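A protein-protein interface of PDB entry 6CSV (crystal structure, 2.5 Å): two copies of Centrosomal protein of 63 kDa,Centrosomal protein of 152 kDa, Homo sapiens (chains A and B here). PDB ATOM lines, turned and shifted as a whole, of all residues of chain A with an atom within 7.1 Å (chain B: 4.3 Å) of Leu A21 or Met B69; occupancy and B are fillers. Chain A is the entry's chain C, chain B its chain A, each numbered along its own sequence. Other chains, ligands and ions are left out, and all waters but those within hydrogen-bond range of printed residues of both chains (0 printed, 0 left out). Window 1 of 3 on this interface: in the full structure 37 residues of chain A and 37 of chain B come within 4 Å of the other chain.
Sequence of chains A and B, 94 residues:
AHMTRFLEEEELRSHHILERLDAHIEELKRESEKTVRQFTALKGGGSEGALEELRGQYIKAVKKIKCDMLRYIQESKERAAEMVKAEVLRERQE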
ATOM      1  N   HIS A  16      26.392 -28.008  16.614  1.00  0.00           N
ATOM      2  CA  HIS A  16      25.558 -28.620  17.682  1.00  0.00           C
ATOM      3  C   HIS A  16      24.538 -27.653  18.252  1.00  0.00           C
ATOM      4  O   HIS A  16      23.352 -27.990  18.344  1.00  0.00           O
ATOM      5  CB  HIS A  16      26.389 -29.288  18.799  1.00  0.00           C
ATOM      6  CG  HIS A  16      27.313 -30.382  18.302  1.00  0.00           C
ATOM      7  ND1 HIS A  16      28.425 -30.807  19.009  1.00  0.00           N
ATOM      8  CD2 HIS A  16      27.319 -31.093  17.142  1.00  0.00           C
ATOM      9  CE1 HIS A  16      29.053 -31.748  18.324  1.00  0.00           C
ATOM     10  NE2 HIS A  16      28.408 -31.933  17.184  1.00  0.00           N
ATOM     11  N   ILE A  17      24.971 -26.444  18.606  1.00  0.00           N
ATOM     12  CA  ILE A  17      24.073 -25.478  19.283  1.00  0.00           C
ATOM     13  C   ILE A  17      22.876 -25.129  18.397  1.00  0.00           C
ATOM     14  O   ILE A  17      21.733 -25.059  18.873  1.00  0.00           O
ATOM     15  CB  ILE A  17      24.829 -24.220  19.822  1.00  0.00           C
ATOM     16  CG1 ILE A  17      23.906 -23.249  20.576  1.00  0.00           C
ATOM     17  CG2 ILE A  17      25.457 -23.444  18.692  1.00  0.00           C
ATOM     18  CD1 ILE A  17      23.398 -23.753  21.900  1.00  0.00           C
ATOM     19  N   LEU A  18      23.120 -24.994  17.105  1.00  0.00           N
ATOM     20  CA  LEU A  18      22.024 -24.755  16.165  1.00  0.00           C
ATOM     21  C   LEU A  18      21.053 -25.966  16.015  1.00  0.00           C
ATOM     22  O   LEU A  18      19.842 -25.768  15.850  1.00  0.00           O
ATOM     23  CB  LEU A  18      22.584 -24.326  14.826  1.00  0.00           C
ATOM     24  CG  LEU A  18      23.434 -23.040  14.957  1.00  0.00           C
ATOM     25  CD1 LEU A  18      24.290 -22.856  13.701  1.00  0.00           C
ATOM     26  CD2 LEU A  18      22.603 -21.787  15.269  1.00  0.00           C
ATOM     27  N   GLU A  19      21.582 -27.190  16.090  1.00  0.00           N
ATOM     28  CA  GLU A  19      20.761 -28.391  16.113  1.00  0.00           C
ATOM     29  C   GLU A  19      19.832 -28.336  17.320  1.00  0.00           C
ATOM     30  O   GLU A  19      18.627 -28.571  17.175  1.00  0.00           O
ATOM     31  CB  GLU A  19      21.590 -29.719  16.132  1.00  0.00           C
ATOM     32  CG  GLU A  19      22.372 -30.030  14.848  1.00  0.00           C
ATOM     33  CD  GLU A  19      23.739 -30.729  15.075  1.00  0.00           C
ATOM     34  OE1 GLU A  19      23.891 -31.526  16.057  1.00  0.00           O
ATOM     35  OE2 GLU A  19      24.684 -30.489  14.257  1.00  0.00           O
ATOM     36  N   ARG A  20      20.357 -28.028  18.501  1.00  0.00           N
ATOM     37  CA  ARG A  20      19.502 -28.076  19.675  1.00  0.00           C
ATOM     38  C   ARG A  20      18.533 -26.850  19.759  1.00  0.00           C
ATOM     39  O   ARG A  20      17.522 -26.923  20.474  1.00  0.00           O
ATOM     40  CB  ARG A  20      20.299 -28.367  20.954  1.00  0.00           C
ATOM     41  CG  ARG A  20      21.134 -27.218  21.486  1.00  0.00           C
ATOM     42  CD  ARG A  20      22.502 -27.679  21.989  1.00  0.00           C
ATOM     43  NE  ARG A  20      22.497 -28.799  22.951  1.00  0.00           N
ATOM     44  CZ  ARG A  20      23.500 -29.679  23.116  1.00  0.00           C
ATOM     45  NH1 ARG A  20      24.613 -29.621  22.365  1.00  0.00           N
ATOM     46  NH2 ARG A  20      23.389 -30.649  24.031  1.00  0.00           N
ATOM     47  N   LEU A  21      18.777 -25.782  18.989  1.00  0.00           N
ATOM     48  CA  LEU A  21      17.752 -24.746  18.814  1.00  0.00           C
ATOM     49  C   LEU A  21      16.640 -25.149  17.855  1.00  0.00           C
ATOM     50  O   LEU A  21      15.484 -24.738  18.064  1.00  0.00           O
ATOM     51  CB  LEU A  21      18.332 -23.416  18.347  1.00  0.00           C
ATOM     52  CG  LEU A  21      19.299 -22.675  19.283  1.00  0.00           C
ATOM     53  CD1 LEU A  21      19.203 -21.198  18.975  1.00  0.00           C
ATOM     54  CD2 LEU A  21      19.101 -22.910  20.790  1.00  0.00           C
ATOM     55  N   ASP A  22      16.972 -25.915  16.804  1.00  0.00           N
ATOM     56  CA  ASP A  22      15.962 -26.432  15.875  1.00  0.00           C
ATOM     57  C   ASP A  22      15.016 -27.418  16.564  1.00  0.00           C
ATOM     58  O   ASP A  22      13.787 -27.423  16.319  1.00  0.00           O
ATOM     59  CB  ASP A  22      16.605 -27.114  14.700  1.00  0.00           C
ATOM     60  CG  ASP A  22      17.361 -26.168  13.815  1.00  0.00           C
ATOM     61  OD1 ASP A  22      16.954 -24.997  13.676  1.00  0.00           O
ATOM     62  OD2 ASP A  22      18.378 -26.608  13.235  1.00  0.00           O
ATOM     63  N   ALA A  23      15.603 -28.218  17.449  1.00  0.00           N
ATOM     64  CA  ALA A  23      14.856 -29.140  18.268  1.00  0.00           C
ATOM     65  C   ALA A  23      13.801 -28.396  19.062  1.00  0.00           C
ATOM     66  O   ALA A  23      12.657 -28.818  19.102  1.00  0.00           O
ATOM     67  CB  ALA A  23      15.787 -29.883  19.201  1.00  0.00           C
ATOM     68  N   HIS A  24      14.192 -27.266  19.645  1.00  0.00           N
ATOM     69  CA  HIS A  24      13.317 -26.494  20.528  1.00  0.00           C
ATOM     70  C   HIS A  24      12.208 -25.817  19.712  1.00  0.00           C
ATOM     71  O   HIS A  24      11.041 -25.901  20.079  1.00  0.00           O
ATOM     72  CB  HIS A  24      14.107 -25.439  21.348  1.00  0.00           C
ATOM     73  CG  HIS A  24      15.219 -25.991  22.210  1.00  0.00           C
ATOM     74  ND1 HIS A  24      15.204 -27.260  22.756  1.00  0.00           N
ATOM     75  CD2 HIS A  24      16.374 -25.417  22.636  1.00  0.00           C
ATOM     76  CE1 HIS A  24      16.311 -27.447  23.458  1.00  0.00           C
ATOM     77  NE2 HIS A  24      17.037 -26.343  23.404  1.00  0.00           N
ATOM     78  N   ILE A  25      12.582 -25.149  18.614  1.00  0.00           N
ATOM     79  CA  ILE A  25      11.606 -24.526  17.712  1.00  0.00           C
ATOM     80  C   ILE A  25      10.531 -25.499  17.266  1.00  0.00           C
ATOM     81  O   ILE A  25       9.345 -25.190  17.347  1.00  0.00           O
ATOM     82  CB  ILE A  25      12.243 -23.927  16.447  1.00  0.00           C
ATOM     83  CG1 ILE A  25      13.263 -22.864  16.833  1.00  0.00           C
ATOM     84  CG2 ILE A  25      11.167 -23.319  15.558  1.00  0.00           C
ATOM     85  CD1 ILE A  25      13.355 -21.649  15.936  1.00  0.00           C
ATOM     86  N   GLU A  26      10.958 -26.671  16.806  1.00  0.00           N
ATOM     87  CA  GLU A  26      10.046 -27.676  16.261  1.00  0.00           C
ATOM     88  C   GLU A  26       9.064 -28.235  17.305  1.00  0.00           C
ATOM     89  O   GLU A  26       7.876 -28.364  17.018  1.00  0.00           O
ATOM     90  CB  GLU A  26      10.858 -28.809  15.604  1.00  0.00           C
ATOM     91  CG  GLU A  26      11.407 -28.461  14.219  1.00  0.00           C
ATOM     92  CD  GLU A  26      10.316 -28.395  13.171  1.00  0.00           C
ATOM     93  OE1 GLU A  26       9.193 -28.887  13.433  1.00  0.00           O
ATOM     94  OE2 GLU A  26      10.573 -27.848  12.076  1.00  0.00           O
ATOM     95  N   GLU A  27       9.559 -28.530  18.508  1.00  0.00           N
ATOM     96  CA  GLU A  27       8.719 -28.933  19.629  1.00  0.00           C
ATOM     97  C   GLU A  27       7.598 -27.902  19.916  1.00  0.00           C
ATOM     98  O   GLU A  27       6.443 -28.274  20.163  1.00  0.00           O
ATOM     99  CB  GLU A  27       9.577 -29.127  20.866  1.00  0.00           C
ATOM    100  CG  GLU A  27       8.857 -29.653  22.086  1.00  0.00           C
ATOM    101  CD  GLU A  27       9.796 -29.731  23.274  1.00  0.00           C
ATOM    102  OE1 GLU A  27      10.801 -28.974  23.287  1.00  0.00           O
ATOM    103  OE2 GLU A  27       9.547 -30.544  24.196  1.00  0.00           O
ATOM    104  N   ALA A  61       9.837 -23.149  25.202  1.00  0.00           N
ATOM    105  CA  ALA A  61      10.805 -23.174  24.126  1.00  0.00           C
ATOM    106  C   ALA A  61      11.869 -22.113  24.368  1.00  0.00           C
ATOM    107  O   ALA A  61      13.057 -22.353  24.121  1.00  0.00           O
ATOM    108  CB  ALA A  61      10.129 -22.986  22.779  1.00  0.00           C
ATOM    109  N   LYS A  64      14.303 -22.990  27.191  1.00  0.00           N
ATOM    110  CA  LYS A  64      15.281 -24.005  26.802  1.00  0.00           C
ATOM    111  C   LYS A  64      16.348 -23.380  25.912  1.00  0.00           C
ATOM    112  O   LYS A  64      17.535 -23.737  25.991  1.00  0.00           O
ATOM    113  CB  LYS A  64      14.593 -25.194  26.142  1.00  0.00           C
ATOM    114  CG  LYS A  64      13.647 -25.913  27.099  1.00  0.00           C
ATOM    115  CD  LYS A  64      13.472 -27.392  26.815  1.00  0.00           C
ATOM    116  CE  LYS A  64      12.492 -27.650  25.684  1.00  0.00           C
ATOM    117  NZ  LYS A  64      12.335 -29.112  25.407  1.00  0.00           N
ATOM    118  N   ILE A  65      15.940 -22.399  25.111  1.00  0.00           N
ATOM    119  CA  ILE A  65      16.891 -21.657  24.301  1.00  0.00           C
ATOM    120  C   ILE A  65      17.827 -20.831  25.176  1.00  0.00           C
ATOM    121  O   ILE A  65      19.010 -20.760  24.895  1.00  0.00           O
ATOM    122  CB  ILE A  65      16.173 -20.827  23.220  1.00  0.00           C
ATOM    123  CG1 ILE A  65      15.590 -21.783  22.172  1.00  0.00           C
ATOM    124  CG2 ILE A  65      17.103 -19.826  22.536  1.00  0.00           C
ATOM    125  CD1 ILE A  65      14.407 -21.219  21.430  1.00  0.00           C
ATOM    126  N   LYS A  66      17.301 -20.247  26.244  1.00  0.00           N
ATOM    127  CA  LYS A  66      18.104 -19.461  27.186  1.00  0.00           C
ATOM    128  C   LYS A  66      19.092 -20.355  27.937  1.00  0.00           C
ATOM    129  O   LYS A  66      20.236 -19.992  28.077  1.00  0.00           O
ATOM    130  CB  LYS A  66      17.199 -18.704  28.160  1.00  0.00           C
ATOM    131  CG  LYS A  66      17.863 -17.571  28.926  1.00  0.00           C
ATOM    132  CD  LYS A  66      17.494 -17.580  30.416  1.00  0.00           C
ATOM    133  CE  LYS A  66      17.952 -16.296  31.113  1.00  0.00           C
ATOM    134  NZ  LYS A  66      17.038 -15.141  30.855  1.00  0.00           N
ATOM    135  N   ASP A  68      20.423 -23.353  26.897  1.00  0.00           N
ATOM    136  CA  ASP A  68      21.443 -23.832  25.955  1.00  0.00           C
ATOM    137  C   ASP A  68      22.419 -22.732  25.531  1.00  0.00           C
ATOM    138  O   ASP A  68      23.623 -22.982  25.369  1.00  0.00           O
ATOM    139  CB  ASP A  68      20.810 -24.487  24.704  1.00  0.00           C
ATOM    140  CG  ASP A  68      20.222 -25.909  24.975  1.00  0.00           C
ATOM    141  OD1 ASP A  68      20.469 -26.483  26.061  1.00  0.00           O
ATOM    142  OD2 ASP A  68      19.502 -26.441  24.087  1.00  0.00           O
ATOM    143  N   MET A  69      21.917 -21.515  25.364  1.00  0.00           N
ATOM    144  CA  MET A  69      22.787 -20.396  25.040  1.00  0.00           C
ATOM    145  C   MET A  69      23.720 -20.014  26.214  1.00  0.00           C
ATOM    146  O   MET A  69      24.892 -19.638  25.985  1.00  0.00           O
ATOM    147  CB  MET A  69      21.986 -19.208  24.513  1.00  0.00           C
ATOM    148  CG  MET A  69      21.663 -19.291  23.014  1.00  0.00           C
ATOM    149  SD  MET A  69      23.068 -19.440  21.853  1.00  0.00           S
ATOM    150  CE  MET A  69      23.833 -17.831  21.659  1.00  0.00           C
ATOM    151  N   TYR A  72      26.553 -22.790  26.244  1.00  0.00           N
ATOM    152  CA  TYR A  72      27.503 -22.431  25.166  1.00  0.00           C
ATOM    153  C   TYR A  72      28.446 -21.311  25.598  1.00  0.00           C
ATOM    154  O   TYR A  72      29.664 -21.478  25.568  1.00  0.00           O
ATOM    155  CB  TYR A  72      26.762 -22.010  23.882  1.00  0.00           C
ATOM    156  CG  TYR A  72      27.631 -21.704  22.650  1.00  0.00           C
ATOM    157  CD1 TYR A  72      28.115 -22.733  21.842  1.00  0.00           C
ATOM    158  CD2 TYR A  72      27.905 -20.377  22.248  1.00  0.00           C
ATOM    159  CE1 TYR A  72      28.879 -22.462  20.700  1.00  0.00           C
ATOM    160  CE2 TYR A  72      28.665 -20.094  21.105  1.00  0.00           C
ATOM    161  CZ  TYR A  72      29.167 -21.140  20.331  1.00  0.00           C
ATOM    162  OH  TYR A  72      29.934 -20.919  19.173  1.00  0.00           O
ATOM    163  N   ILE A  73      27.855 -20.191  26.015  1.00  0.00           N
ATOM    164  CA  ILE A  73      28.585 -19.015  26.469  1.00  0.00           C
ATOM    165  C   ILE A  73      29.600 -19.353  27.550  1.00  0.00           C
ATOM    166  O   ILE A  73      30.778 -19.105  27.361  1.00  0.00           O
ATOM    167  CB  ILE A  73      27.578 -17.956  26.939  1.00  0.00           C
ATOM    168  CG1 ILE A  73      26.980 -17.281  25.707  1.00  0.00           C
ATOM    169  CG2 ILE A  73      28.217 -16.935  27.866  1.00  0.00           C
ATOM    170  CD1 ILE A  73      25.589 -16.733  25.884  1.00  0.00           C
ATOM    171  N   ILE B  17      25.024 -10.230  24.206  1.00  0.00           N
ATOM    172  CA  ILE B  17      24.012 -11.118  23.613  1.00  0.00           C
ATOM    173  C   ILE B  17      22.903 -11.475  24.622  1.00  0.00           C
ATOM    174  O   ILE B  17      21.735 -11.530  24.257  1.00  0.00           O
ATOM    175  CB  ILE B  17      24.639 -12.390  22.953  1.00  0.00           C
ATOM    176  CG1 ILE B  17      23.700 -13.001  21.900  1.00  0.00           C
ATOM    177  CG2 ILE B  17      24.979 -13.470  23.967  1.00  0.00           C
ATOM    178  CD1 ILE B  17      23.477 -12.135  20.667  1.00  0.00           C
ATOM    179  N   ILE B  65      14.846 -15.103  17.771  1.00  0.00           N
ATOM    180  CA  ILE B  65      15.859 -15.450  18.755  1.00  0.00           C
ATOM    181  C   ILE B  65      16.931 -16.299  18.093  1.00  0.00           C
ATOM    182  O   ILE B  65      18.092 -15.931  18.135  1.00  0.00           O
ATOM    183  CB  ILE B  65      15.230 -16.124  19.981  1.00  0.00           C
ATOM    184  CG1 ILE B  65      14.554 -15.038  20.806  1.00  0.00           C
ATOM    185  CG2 ILE B  65      16.260 -16.869  20.825  1.00  0.00           C
ATOM    186  CD1 ILE B  65      13.319 -15.499  21.506  1.00  0.00           C
ATOM    187  N   LYS B  66      16.549 -17.389  17.436  1.00  0.00           N
ATOM    188  CA  LYS B  66      17.514 -18.190  16.665  1.00  0.00           C
ATOM    189  C   LYS B  66      18.368 -17.332  15.702  1.00  0.00           C
ATOM    190  O   LYS B  66      19.578 -17.422  15.702  1.00  0.00           O
ATOM    191  CB  LYS B  66      16.798 -19.316  15.904  1.00  0.00           C
ATOM    192  CG  LYS B  66      17.739 -20.308  15.185  1.00  0.00           C
ATOM    193  CD  LYS B  66      16.963 -21.259  14.275  1.00  0.00           C
ATOM    194  CE  LYS B  66      17.674 -21.561  12.964  1.00  0.00           C
ATOM    195  NZ  LYS B  66      16.680 -21.939  11.923  1.00  0.00           N
ATOM    196  N   CYS B  67      17.743 -16.478  14.917  1.00  0.00           N
ATOM    197  CA  CYS B  67      18.486 -15.618  13.991  1.00  0.00           C
ATOM    198  C   CYS B  67      19.535 -14.755  14.635  1.00  0.00           C
ATOM    199  O   CYS B  67      20.613 -14.596  14.076  1.00  0.00           O
ATOM    200  CB  CYS B  67      17.556 -14.753  13.131  1.00  0.00           C
ATOM    201  SG  CYS B  67      16.758 -15.768  11.861  1.00  0.00           S
ATOM    202  N   ASP B  68      19.243 -14.213  15.816  1.00  0.00           N
ATOM    203  CA  ASP B  68      20.275 -13.511  16.618  1.00  0.00           C
ATOM    204  C   ASP B  68      21.315 -14.481  17.174  1.00  0.00           C
ATOM    205  O   ASP B  68      22.501 -14.170  17.193  1.00  0.00           O
ATOM    206  CB  ASP B  68      19.644 -12.660  17.724  1.00  0.00           C
ATOM    207  CG  ASP B  68      18.814 -11.517  17.162  1.00  0.00           C
ATOM    208  OD1 ASP B  68      19.399 -10.629  16.508  1.00  0.00           O
ATOM    209  OD2 ASP B  68      17.576 -11.495  17.359  1.00  0.00           O
ATOM    210  N   MET B  69      20.898 -15.671  17.590  1.00  0.00           N
ATOM    211  CA  MET B  69      21.858 -16.633  18.084  1.00  0.00           C
ATOM    212  C   MET B  69      22.773 -17.141  16.988  1.00  0.00           C
ATOM    213  O   MET B  69      23.948 -17.316  17.238  1.00  0.00           O
ATOM    214  CB  MET B  69      21.153 -17.769  18.804  1.00  0.00           C
ATOM    215  CG  MET B  69      20.306 -17.317  20.006  1.00  0.00           C
ATOM    216  SD  MET B  69      21.042 -16.117  21.172  1.00  0.00           S
ATOM    217  CE  MET B  69      20.393 -14.520  20.632  1.00  0.00           C
ATOM    218  N   LEU B  70      22.264 -17.341  15.764  1.00  0.00           N
ATOM    219  CA  LEU B  70      23.134 -17.661  14.613  1.00  0.00           C
ATOM    220  C   LEU B  70      24.172 -16.600  14.334  1.00  0.00           C
ATOM    221  O   LEU B  70      25.322 -16.923  14.073  1.00  0.00           O
ATOM    222  CB  LEU B  70      22.340 -17.844  13.319  1.00  0.00           C
ATOM    223  CG  LEU B  70      21.843 -19.254  13.025  1.00  0.00           C
ATOM    224  CD1 LEU B  70      20.707 -19.199  12.020  1.00  0.00           C
ATOM    225  CD2 LEU B  70      22.963 -20.106  12.480  1.00  0.00           C
ATOM    226  N   ARG B  71      23.763 -15.331  14.342  1.00  0.00           N
ATOM    227  CA  ARG B  71      24.712 -14.222  14.122  1.00  0.00           C
ATOM    228  C   ARG B  71      25.828 -14.248  15.172  1.00  0.00           C
ATOM    229  O   ARG B  71      27.003 -14.063  14.831  1.00  0.00           O
ATOM    230  CB  ARG B  71      24.028 -12.863  14.152  1.00  0.00           C
ATOM    231  CG  ARG B  71      23.044 -12.607  13.027  1.00  0.00           C
ATOM    232  CD  ARG B  71      22.645 -11.123  12.973  1.00  0.00           C
ATOM    233  NE  ARG B  71      21.196 -10.929  13.076  1.00  0.00           N
ATOM    234  CZ  ARG B  71      20.311 -11.123  12.093  1.00  0.00           C
ATOM    235  NH1 ARG B  71      20.693 -11.523  10.872  1.00  0.00           N
ATOM    236  NH2 ARG B  71      19.017 -10.911  12.328  1.00  0.00           N
ATOM    237  N   TYR B  72      25.468 -14.495  16.431  1.00  0.00           N
ATOM    238  CA  TYR B  72      26.466 -14.569  17.488  1.00  0.00           C
ATOM    239  C   TYR B  72      27.487 -15.674  17.206  1.00  0.00           C
ATOM    240  O   TYR B  72      28.690 -15.453  17.252  1.00  0.00           O
ATOM    241  CB  TYR B  72      25.797 -14.816  18.849  1.00  0.00           C
ATOM    242  CG  TYR B  72      26.747 -14.789  20.001  1.00  0.00           C
ATOM    243  CD1 TYR B  72      27.292 -13.619  20.407  1.00  0.00           C
ATOM    244  CD2 TYR B  72      27.095 -15.937  20.674  1.00  0.00           C
ATOM    245  CE1 TYR B  72      28.159 -13.564  21.486  1.00  0.00           C
ATOM    246  CE2 TYR B  72      27.965 -15.909  21.756  1.00  0.00           C
ATOM    247  CZ  TYR B  72      28.510 -14.706  22.163  1.00  0.00           C
ATOM    248  OH  TYR B  72      29.402 -14.616  23.223  1.00  0.00           O
ATOM    249  N   ILE B  73      26.977 -16.866  16.950  1.00  0.00           N
ATOM    250  CA  ILE B  73      27.819 -18.002  16.616  1.00  0.00           C
ATOM    251  C   ILE B  73      28.693 -17.679  15.409  1.00  0.00           C
ATOM    252  O   ILE B  73      29.915 -17.910  15.437  1.00  0.00           O
ATOM    253  CB  ILE B  73      26.981 -19.243  16.225  1.00  0.00           C
ATOM    254  CG1 ILE B  73      26.070 -19.712  17.355  1.00  0.00           C
ATOM    255  CG2 ILE B  73      27.870 -20.360  15.763  1.00  0.00           C
ATOM    256  CD1 ILE B  73      26.792 -20.200  18.543  1.00  0.00           C
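NZ of Lys B66 is in salt-bridge range of OD1 of Asp A22 (3.5 Å).
Among the printed residues, pairs that only touch across the chains: Ile A17 with Ile B73 (3.5 Å), Leu A18 with Leu B70 (3.3 Å), Leu A21 with Met B69 (3.9 Å), Ile A25 with Lys B66 (3.99 Å), Ile A65 with Ile B65 (3.5 Å), Met A69 with Met B69 (3.3 Å), Met A69 with Tyr B72 (3.9 Å), Tyr A72 with Ile B73 (3.1 Å) and Ile A73 with Ile B17 (3.8 Å).
Of chain B, only Met B69 (3.9 Å) comes within 4 Å of Leu A21. Of the printed residues of chain B, Ile A25 touches Lys B66 (3.99 Å). Ala A61 touches none of the printed residues of chain B. Asp A68 touches none of the printed residues of chain B. Of the printed residues of chain B, Tyr A72 touches Ile B73. Met B69 touches just these residues of chain A: Leu A21 (3.9 Å) and Met A69 (3.3 Å). Printed residues of chain A within 4 Å of Leu B70: Leu A18. The nearest residue of chain B that does not touch Leu A21 is Lys B66 (4.2 Å). The nearest residue of chain A that does not touch Met B69 is Ile A65 (4.8 Å). The nearest printed residue of chain B that does not touch Ile A25 is Ile B65 (6.8 Å).
Of the 20 printed residues of chain A, 9 touch a printed residue of chain B. Printed residues of chain A that touch a printed residue of chain B: Ile A17, Leu A18, Leu A21, Asp A22, Ile A25, Ile A65, Met A69, Tyr A72 and Ile A73. Hydrophobic or aromatic side chains of chain A within 4 Å of the printed part of chain B: Ile A17, Leu A18, Leu A21, Ile A25, Ile A65, Met A69, Tyr A72 and Ile A73. Of the 10 printed residues of chain B, 7 touch a printed residue of chain A. Hydrophobic or aromatic side chains of chain B within 4 Å of the printed part of chain A: Ile B17, Ile B65, Met B69, Leu B70, Tyr B72 and Ile B73. Among the printed residues, Asp or Glu carboxylates within 4 Å of a Lys or Arg side-chain nitrogen of the other chain: Asp A22 with Lys B66 (3.5 Å).
Ile A17 touches Ile B73, and with the chains exchanged Ile A73 touches Ile B17. Ile A65 touches its own counterpart, Ile B65. Met B69 touches its own counterpart, Met A69. Tyr A72 touches Ile B73, but with the chains exchanged Ile A73 does not touch Tyr B72 (4.3 Å). Positions printed for both chains: 17, 65, 66, 68, 69, 72 and 73. Of the 10 pairs that touch across the chains among the printed residues, 4 have their exchanged pair printed and touching as well.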
